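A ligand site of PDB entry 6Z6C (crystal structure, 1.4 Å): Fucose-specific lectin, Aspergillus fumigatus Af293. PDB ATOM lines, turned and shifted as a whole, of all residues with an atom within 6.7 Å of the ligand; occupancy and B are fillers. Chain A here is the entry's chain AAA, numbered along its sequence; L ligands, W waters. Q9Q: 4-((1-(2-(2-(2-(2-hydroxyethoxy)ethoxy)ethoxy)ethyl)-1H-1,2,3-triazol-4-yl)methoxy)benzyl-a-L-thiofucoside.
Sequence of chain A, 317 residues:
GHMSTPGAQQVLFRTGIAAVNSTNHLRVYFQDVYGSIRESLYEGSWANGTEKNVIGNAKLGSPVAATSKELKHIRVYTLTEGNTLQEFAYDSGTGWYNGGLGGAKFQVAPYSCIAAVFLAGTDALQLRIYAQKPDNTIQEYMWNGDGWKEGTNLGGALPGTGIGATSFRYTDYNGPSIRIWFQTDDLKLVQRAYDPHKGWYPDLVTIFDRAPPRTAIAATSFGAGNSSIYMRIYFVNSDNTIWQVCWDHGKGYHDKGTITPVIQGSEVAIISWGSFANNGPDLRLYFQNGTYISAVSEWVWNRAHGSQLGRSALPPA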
ATOM      1  N   VAL A  20       9.874  -1.908 -25.625  1.00  0.00           N
ATOM      2  CA  VAL A  20       8.980  -0.771 -25.254  1.00  0.00           C
ATOM      3  C   VAL A  20       9.817   0.491 -25.201  1.00  0.00           C
ATOM      4  O   VAL A  20      11.055   0.450 -25.163  1.00  0.00           O
ATOM      5  CB  VAL A  20       8.287  -1.032 -23.896  1.00  0.00           C
ATOM      6  CG1 VAL A  20       7.440  -2.288 -23.913  1.00  0.00           C
ATOM      7  CG2 VAL A  20       9.283  -1.078 -22.744  1.00  0.00           C
ATOM      8  N   ASN A  21       9.158   1.626 -25.087  1.00  0.00           N
ATOM      9  CA  ASN A  21       9.828   2.924 -25.128  1.00  0.00           C
ATOM     10  C   ASN A  21       8.918   4.032 -24.592  1.00  0.00           C
ATOM     11  O   ASN A  21       7.704   3.950 -24.649  1.00  0.00           O
ATOM     12  CB  ASN A  21      10.351   3.232 -26.537  1.00  0.00           C
ATOM     13  CG  ASN A  21       9.220   3.491 -27.520  1.00  0.00           C
ATOM     14  OD1 ASN A  21       8.365   2.602 -27.703  1.00  0.00           O
ATOM     15  ND2 ASN A  21       9.227   4.652 -28.154  1.00  0.00           N
ATOM     16  N   SER A  22       9.565   5.084 -24.173  1.00  0.00           N
ATOM     17  CA  SER A  22       9.040   6.447 -24.098  1.00  0.00           C
ATOM     18  C   SER A  22       9.953   7.301 -24.965  1.00  0.00           C
ATOM     19  O   SER A  22      11.084   7.456 -24.567  1.00  0.00           O
ATOM     20  CB  SER A  22       8.992   6.974 -22.688  1.00  0.00           C
ATOM     21  OG  SER A  22       8.369   8.228 -22.671  1.00  0.00           O
ATOM     22  N   THR A  23       9.479   7.755 -26.120  1.00  0.00           N
ATOM     23  CA  THR A  23      10.333   8.352 -27.182  1.00  0.00           C
ATOM     24  C   THR A  23      11.633   7.553 -27.245  1.00  0.00           C
ATOM     25  O   THR A  23      11.545   6.320 -27.491  1.00  0.00           O
ATOM     26  CB  THR A  23      10.527   9.877 -27.012  1.00  0.00           C
ATOM     27  OG1 THR A  23      11.252  10.231 -25.833  1.00  0.00           O
ATOM     28  CG2 THR A  23       9.206  10.630 -27.025  1.00  0.00           C
ATOM     29  N   HIS A  25      13.813   6.633 -25.039  1.00  0.00           N
ATOM     30  CA  HIS A  25      14.149   5.870 -23.827  1.00  0.00           C
ATOM     31  C   HIS A  25      13.668   4.433 -24.002  1.00  0.00           C
ATOM     32  O   HIS A  25      12.463   4.264 -24.142  1.00  0.00           O
ATOM     33  CB  HIS A  25      13.494   6.485 -22.587  1.00  0.00           C
ATOM     34  CG  HIS A  25      13.776   7.965 -22.420  1.00  0.00           C
ATOM     35  ND1 HIS A  25      14.797   8.460 -21.645  1.00  0.00           N
ATOM     36  CD2 HIS A  25      13.190   9.043 -22.987  1.00  0.00           C
ATOM     37  CE1 HIS A  25      14.792   9.778 -21.696  1.00  0.00           C
ATOM     38  NE2 HIS A  25      13.836  10.163 -22.526  1.00  0.00           N
ATOM     39  N   LEU A  26      14.543   3.455 -24.214  1.00  0.00           N
ATOM     40  CA  LEU A  26      14.149   2.150 -24.778  1.00  0.00           C
ATOM     41  C   LEU A  26      14.411   1.031 -23.773  1.00  0.00           C
ATOM     42  O   LEU A  26      15.415   1.088 -22.978  1.00  0.00           O
ATOM     43  CB  LEU A  26      15.005   1.866 -26.028  1.00  0.00           C
ATOM     44  CG  LEU A  26      15.264   2.999 -26.997  1.00  0.00           C
ATOM     45  CD1 LEU A  26      16.127   2.527 -28.157  1.00  0.00           C
ATOM     46  CD2 LEU A  26      14.014   3.639 -27.540  1.00  0.00           C
ATOM     47  N   ARG A  27      13.636  -0.018 -23.877  1.00  0.00           N
ATOM     48  CA  ARG A  27      13.836  -1.273 -23.142  1.00  0.00           C
ATOM     49  C   ARG A  27      13.666  -2.397 -24.151  1.00  0.00           C
ATOM     50  O   ARG A  27      12.695  -2.403 -24.913  1.00  0.00           O
ATOM     51  CB  ARG A  27      12.905  -1.447 -21.940  1.00  0.00           C
ATOM     52  CG  ARG A  27      12.910  -0.286 -20.953  1.00  0.00           C
ATOM     53  CD  ARG A  27      14.218  -0.160 -20.193  1.00  0.00           C
ATOM     54  NE  ARG A  27      14.182   0.913 -19.195  1.00  0.00           N
ATOM     55  CZ  ARG A  27      14.505   2.185 -19.406  1.00  0.00           C
ATOM     56  NH1 ARG A  27      14.907   2.624 -20.587  1.00  0.00           N
ATOM     57  NH2 ARG A  27      14.423   3.042 -18.386  1.00  0.00           N
ATOM     58  N   TYR A  29      13.632  -6.749 -24.312  1.00  0.00           N
ATOM     59  CA  TYR A  29      13.489  -8.003 -23.542  1.00  0.00           C
ATOM     60  C   TYR A  29      13.817  -9.182 -24.456  1.00  0.00           C
ATOM     61  O   TYR A  29      13.434  -9.210 -25.630  1.00  0.00           O
ATOM     62  CB  TYR A  29      12.065  -8.157 -23.001  1.00  0.00           C
ATOM     63  CG  TYR A  29      11.676  -6.989 -22.155  1.00  0.00           C
ATOM     64  CD1 TYR A  29      12.156  -6.829 -20.876  1.00  0.00           C
ATOM     65  CD2 TYR A  29      10.949  -5.928 -22.694  1.00  0.00           C
ATOM     66  CE1 TYR A  29      11.898  -5.694 -20.126  1.00  0.00           C
ATOM     67  CE2 TYR A  29      10.666  -4.807 -21.957  1.00  0.00           C
ATOM     68  CZ  TYR A  29      11.160  -4.674 -20.678  1.00  0.00           C
ATOM     69  OH  TYR A  29      10.997  -3.513 -19.989  1.00  0.00           O
ATOM     70  N   GLU A  39      16.369  -7.775 -19.427  1.00  0.00           N
ATOM     71  CA  GLU A  39      16.083  -6.439 -19.941  1.00  0.00           C
ATOM     72  C   GLU A  39      17.388  -5.714 -20.260  1.00  0.00           C
ATOM     73  O   GLU A  39      18.244  -5.530 -19.343  1.00  0.00           O
ATOM     74  CB  GLU A  39      15.293  -5.648 -18.913  1.00  0.00           C
ATOM     75  CG  GLU A  39      14.885  -4.274 -19.403  1.00  0.00           C
ATOM     76  CD  GLU A  39      14.325  -3.396 -18.287  1.00  0.00           C
ATOM     77  OE1 GLU A  39      15.038  -3.016 -17.391  1.00  0.00           O
ATOM     78  OE2 GLU A  39      13.100  -3.033 -18.385  1.00  0.00           O
ATOM     79  N   LEU A  41      18.719  -1.915 -21.741  1.00  0.00           N
ATOM     80  CA  LEU A  41      18.139  -0.559 -21.728  1.00  0.00           C
ATOM     81  C   LEU A  41      18.990   0.445 -22.448  1.00  0.00           C
ATOM     82  O   LEU A  41      20.192   0.306 -22.533  1.00  0.00           O
ATOM     83  CB  LEU A  41      17.629  -0.104 -20.383  1.00  0.00           C
ATOM     84  CG  LEU A  41      18.578   0.389 -19.330  1.00  0.00           C
ATOM     85  CD1 LEU A  41      19.312   1.707 -19.607  1.00  0.00           C
ATOM     86  CD2 LEU A  41      17.809   0.572 -18.023  1.00  0.00           C
ATOM     87  N   GLU A  43      19.256   4.502 -22.182  1.00  0.00           N
ATOM     88  CA  GLU A  43      19.028   5.854 -21.602  1.00  0.00           C
ATOM     89  C   GLU A  43      20.241   6.700 -22.012  1.00  0.00           C
ATOM     90  O   GLU A  43      21.067   7.026 -21.154  1.00  0.00           O
ATOM     91  CB  GLU A  43      18.859   5.766 -20.085  1.00  0.00           C
ATOM     92  CG  GLU A  43      17.559   5.090 -19.648  1.00  0.00           C
ATOM     93  CD  GLU A  43      16.339   5.928 -19.921  1.00  0.00           C
ATOM     94  OE1 GLU A  43      16.506   7.165 -20.111  1.00  0.00           O
ATOM     95  OE2 GLU A  43      15.230   5.359 -19.947  1.00  0.00           O
ATOM     96  N   ASN A  48      22.902  -2.891 -19.356  1.00  0.00           N
ATOM     97  CA  ASN A  48      22.207  -4.017 -18.710  1.00  0.00           C
ATOM     98  C   ASN A  48      22.219  -5.259 -19.582  1.00  0.00           C
ATOM     99  O   ASN A  48      23.247  -5.561 -20.173  1.00  0.00           O
ATOM    100  CB  ASN A  48      20.849  -3.550 -18.182  1.00  0.00           C
ATOM    101  CG  ASN A  48      20.981  -2.513 -17.076  1.00  0.00           C
ATOM    102  OD1 ASN A  48      19.962  -1.936 -16.607  1.00  0.00           O
ATOM    103  ND2 ASN A  48      22.189  -2.284 -16.599  1.00  0.00           N
ATOM    104  N   ASN A  53      19.968  -8.473 -14.492  1.00  0.00           N
ATOM    105  CA  ASN A  53      18.845  -7.734 -15.135  1.00  0.00           C
ATOM    106  C   ASN A  53      17.738  -8.699 -15.539  1.00  0.00           C
ATOM    107  O   ASN A  53      17.088  -8.461 -16.561  1.00  0.00           O
ATOM    108  CB  ASN A  53      19.369  -6.882 -16.290  1.00  0.00           C
ATOM    109  CG  ASN A  53      20.568  -6.049 -15.879  1.00  0.00           C
ATOM    110  OD1 ASN A  53      21.664  -6.258 -16.404  1.00  0.00           O
ATOM    111  ND2 ASN A  53      20.410  -5.142 -14.914  1.00  0.00           N
ATOM    112  N   ILE A  55      14.078 -10.351 -15.146  1.00  0.00           N
ATOM    113  CA  ILE A  55      12.734  -9.944 -14.645  1.00  0.00           C
ATOM    114  C   ILE A  55      11.822 -11.141 -14.407  1.00  0.00           C
ATOM    115  O   ILE A  55      10.719 -10.958 -13.831  1.00  0.00           O
ATOM    116  CB  ILE A  55      12.097  -8.930 -15.604  1.00  0.00           C
ATOM    117  CG1 ILE A  55      11.825  -9.501 -17.008  1.00  0.00           C
ATOM    118  CG2 ILE A  55      12.920  -7.665 -15.629  1.00  0.00           C
ATOM    119  CD1 ILE A  55      10.873  -8.651 -17.844  1.00  0.00           C
ATOM    120  N   GLU A  70       4.321   4.730 -21.737  1.00  0.00           N
ATOM    121  CA  GLU A  70       5.646   5.368 -21.643  1.00  0.00           C
ATOM    122  C   GLU A  70       6.543   4.353 -20.906  1.00  0.00           C
ATOM    123  O   GLU A  70       6.541   3.186 -21.298  1.00  0.00           O
ATOM    124  CB  GLU A  70       5.518   6.772 -21.068  1.00  0.00           C
ATOM    125  CG  GLU A  70       4.546   7.635 -21.848  1.00  0.00           C
ATOM    126  CD  GLU A  70       4.838   7.889 -23.331  1.00  0.00           C
ATOM    127  OE1 GLU A  70       5.987   7.832 -23.750  1.00  0.00           O
ATOM    128  OE2 GLU A  70       3.862   8.152 -24.080  1.00  0.00           O
ATOM    129  N   LEU A  71       7.294   4.776 -19.906  1.00  0.00           N
ATOM    130  CA  LEU A  71       8.031   3.768 -19.093  1.00  0.00           C
ATOM    131  C   LEU A  71       7.526   3.842 -17.659  1.00  0.00           C
ATOM    132  O   LEU A  71       8.202   3.390 -16.746  1.00  0.00           O
ATOM    133  CB  LEU A  71       9.541   3.959 -19.171  1.00  0.00           C
ATOM    134  CG  LEU A  71      10.144   3.778 -20.570  1.00  0.00           C
ATOM    135  CD1 LEU A  71      11.606   4.103 -20.522  1.00  0.00           C
ATOM    136  CD2 LEU A  71       9.983   2.370 -21.055  1.00  0.00           C
ATOM    137  N   LYS A  72       6.308   4.312 -17.477  1.00  0.00           N
ATOM    138  CA  LYS A  72       5.666   4.348 -16.143  1.00  0.00           C
ATOM    139  C   LYS A  72       5.095   2.969 -15.799  1.00  0.00           C
ATOM    140  O   LYS A  72       5.114   2.559 -14.656  1.00  0.00           O
ATOM    141  CB  LYS A  72       4.588   5.432 -16.146  1.00  0.00           C
ATOM    142  CG  LYS A  72       3.951   5.628 -14.781  1.00  0.00           C
ATOM    143  CD  LYS A  72       2.940   6.725 -14.752  1.00  0.00           C
ATOM    144  CE  LYS A  72       2.508   6.950 -13.318  1.00  0.00           C
ATOM    145  NZ  LYS A  72       1.337   7.850 -13.270  1.00  0.00           N
ATOM    146  N   ILE A  74       5.070  -1.063 -17.427  1.00  0.00           N
ATOM    147  CA  ILE A  74       5.534  -2.013 -18.474  1.00  0.00           C
ATOM    148  C   ILE A  74       4.959  -3.383 -18.130  1.00  0.00           C
ATOM    149  O   ILE A  74       4.929  -3.740 -16.937  1.00  0.00           O
ATOM    150  CB  ILE A  74       7.080  -2.085 -18.510  1.00  0.00           C
ATOM    151  CG1 ILE A  74       7.717  -0.693 -18.673  1.00  0.00           C
ATOM    152  CG2 ILE A  74       7.519  -3.083 -19.597  1.00  0.00           C
ATOM    153  CD1 ILE A  74       9.238  -0.708 -18.463  1.00  0.00           C
ATOM    154  N   TYR A  90       6.037  -3.998 -14.268  1.00  0.00           N
ATOM    155  CA  TYR A  90       6.803  -2.882 -13.685  1.00  0.00           C
ATOM    156  C   TYR A  90       5.854  -1.695 -13.554  1.00  0.00           C
ATOM    157  O   TYR A  90       5.211  -1.362 -14.557  1.00  0.00           O
ATOM    158  CB  TYR A  90       7.987  -2.517 -14.562  1.00  0.00           C
ATOM    159  CG  TYR A  90       8.717  -1.297 -14.072  1.00  0.00           C
ATOM    160  CD1 TYR A  90       9.745  -1.441 -13.138  1.00  0.00           C
ATOM    161  CD2 TYR A  90       8.363  -0.018 -14.476  1.00  0.00           C
ATOM    162  CE1 TYR A  90      10.381  -0.314 -12.628  1.00  0.00           C
ATOM    163  CE2 TYR A  90       9.004   1.099 -13.980  1.00  0.00           C
ATOM    164  CZ  TYR A  90      10.041   0.949 -13.082  1.00  0.00           C
ATOM    165  OH  TYR A  90      10.673   2.028 -12.528  1.00  0.00           O
ATOM    166  N   SER A  92       6.270   2.415 -12.063  1.00  0.00           N
ATOM    167  CA  SER A  92       7.119   3.440 -11.424  1.00  0.00           C
ATOM    168  C   SER A  92       6.812   3.460  -9.933  1.00  0.00           C
ATOM    169  O   SER A  92       5.616   3.537  -9.599  1.00  0.00           O
ATOM    170  CB  SER A  92       6.842   4.780 -12.024  1.00  0.00           C
ATOM    171  OG  SER A  92       7.409   4.830 -13.315  1.00  0.00           O
ATOM    172  N   TRP A  96       9.573  -4.184 -10.294  1.00  0.00           N
ATOM    173  CA  TRP A  96       9.103  -5.416 -10.957  1.00  0.00           C
ATOM    174  C   TRP A  96       8.402  -6.328  -9.970  1.00  0.00           C
ATOM    175  O   TRP A  96       8.861  -6.508  -8.821  1.00  0.00           O
ATOM    176  CB  TRP A  96      10.282  -6.136 -11.626  1.00  0.00           C
ATOM    177  CG  TRP A  96      10.771  -5.439 -12.847  1.00  0.00           C
ATOM    178  CD1 TRP A  96      11.827  -4.593 -12.912  1.00  0.00           C
ATOM    179  CD2 TRP A  96      10.212  -5.481 -14.155  1.00  0.00           C
ATOM    180  NE1 TRP A  96      12.001  -4.140 -14.191  1.00  0.00           N
ATOM    181  CE2 TRP A  96      10.991  -4.640 -14.973  1.00  0.00           C
ATOM    182  CE3 TRP A  96       9.123  -6.145 -14.731  1.00  0.00           C
ATOM    183  CZ2 TRP A  96      10.704  -4.428 -16.320  1.00  0.00           C
ATOM    184  CZ3 TRP A  96       8.851  -5.959 -16.064  1.00  0.00           C
ATOM    185  CH2 TRP A  96       9.642  -5.123 -16.847  1.00  0.00           C
HETATM  186  C19 Q9Q L   1      10.604  11.389 -20.495  1.00  0.00           C
HETATM  187  N3  Q9Q L   1      11.193  10.109 -20.036  1.00  0.00           N
HETATM  188  N2  Q9Q L   1      10.403   8.995 -20.166  1.00  0.00           N
HETATM  189  C18 Q9Q L   1      12.325   9.655 -19.445  1.00  0.00           C
HETATM  190  C17 Q9Q L   1      12.221   8.237 -19.267  1.00  0.00           C
HETATM  191  N1  Q9Q L   1      11.001   7.832 -19.746  1.00  0.00           N
HETATM  192  C16 Q9Q L   1      13.214   7.238 -18.661  1.00  0.00           C
HETATM  193  O6  Q9Q L   1      12.688   6.859 -17.420  1.00  0.00           O
HETATM  194  C13 Q9Q L   1      13.398   6.108 -16.549  1.00  0.00           C
HETATM  195  C12 Q9Q L   1      12.677   5.490 -15.604  1.00  0.00           C
HETATM  196  C11 Q9Q L   1      13.327   4.754 -14.682  1.00  0.00           C
HETATM  197  C14 Q9Q L   1      14.764   5.954 -16.562  1.00  0.00           C
HETATM  198  C15 Q9Q L   1      15.420   5.175 -15.638  1.00  0.00           C
HETATM  199  C10 Q9Q L   1      14.678   4.569 -14.665  1.00  0.00           C
HETATM  200  C9  Q9Q L   1      15.184   3.668 -13.562  1.00  0.00           C
HETATM  201  S1  Q9Q L   1      14.493   2.011 -13.390  1.00  0.00           S
HETATM  202  C1  Q9Q L   1      14.694   1.403 -15.144  1.00  0.00           C
HETATM  203  O5  Q9Q L   1      13.617   1.804 -15.970  1.00  0.00           O
HETATM  204  C5  Q9Q L   1      12.417   1.099 -15.720  1.00  0.00           C
HETATM  205  C6  Q9Q L   1      11.400   1.769 -16.548  1.00  0.00           C
HETATM  206  C4  Q9Q L   1      12.516  -0.408 -15.901  1.00  0.00           C
HETATM  207  O4  Q9Q L   1      12.789  -0.569 -17.302  1.00  0.00           O
HETATM  208  C3  Q9Q L   1      13.643  -0.883 -14.997  1.00  0.00           C
HETATM  209  O3  Q9Q L   1      13.928  -2.225 -15.162  1.00  0.00           O
HETATM  210  C2  Q9Q L   1      14.894  -0.073 -15.217  1.00  0.00           C
HETATM  211  O2  Q9Q L   1      15.911  -0.505 -14.302  1.00  0.00           O
HETATM  212  O   HOH W   1       9.803  10.382 -23.523  1.00  0.00           O
HETATM  213  O   HOH W   2      12.681  12.819 -22.654  1.00  0.00           O
HETATM  214  O   HOH W   3       7.988   7.314 -18.723  1.00  0.00           O
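The side-chain carboxylate (OE1) of Glu 39 lies within hydrogen-bond range of an oxygen (O3) of the ligand (2.6 Å). The side-chain hydroxyl (OG) of Ser 22 is in hydrogen-bond range of a nitrogen (N2) of the ligand, at 3.3 Å. The indole nitrogen (NE1) of Trp 96 sits at hydrogen-bond distance from an oxygen (O3) of the ligand (2.9 Å). The guanidinium group (NE) of Arg 27 is in hydrogen-bond range of an oxygen (O4) of the ligand (2.8 Å).
The backbone NH of Ile 74 lies within hydrogen-bond range of the backbone carbonyl oxygen of Tyr 90. The side-chain carboxylate (OE1) of Glu 43 lies within hydrogen-bond range of a ring nitrogen (ND1) of His 25. N of Arg 27 is in hydrogen-bond range of O of Val 20. The backbone NH (N) of Glu 39 sits at hydrogen-bond distance from the backbone carbonyl oxygen (O) of Asn 53, 3.0 Å away. OE2 of Glu 39 sits at hydrogen-bond distance from OH of Tyr 29, 2.7 Å away. The guanidinium group of Arg 27 is in salt-bridge range of the side-chain carboxylate of Glu 43 (2.8 Å). The side-chain carboxylate (OE1) of Glu 70 sits at hydrogen-bond distance from the side-chain hydroxyl (OG) of Ser 22 (2.6 Å).
CE1 of His 25 touches C18 of the ligand, at 3.3 Å. OE2 of Glu 43 touches C16 of the ligand, at 3.0 Å. O of Leu 71 touches C6 of the ligand, 3.6 Å away. Ile 74 touches the ligand. CZ of Tyr 90 touches C5 of the ligand (3.6 Å). Hydrophobic or aromatic side chains that line the ligand: His 25, Leu 71, Ile 74, Tyr 90 and Trp 96. Of the 21 residues printed, 9 come within 4 Å of the ligand. Along chain A the residues within 4 Å of the ligand span positions 22 to 96. The nearest printed residue that does not touch the ligand is Leu 41 (4.1 Å).
Water W3 lies within hydrogen-bond range of the backbone NH of Leu 71 (2.9 Å) and a nitrogen (N1) of the ligand (3.2 Å). Water W1 lies within hydrogen-bond range of the side-chain hydroxyl (OG) of Ser 22 (2.7 Å) and the side-chain hydroxyl (OG1) of Thr 23 (2.7 Å).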
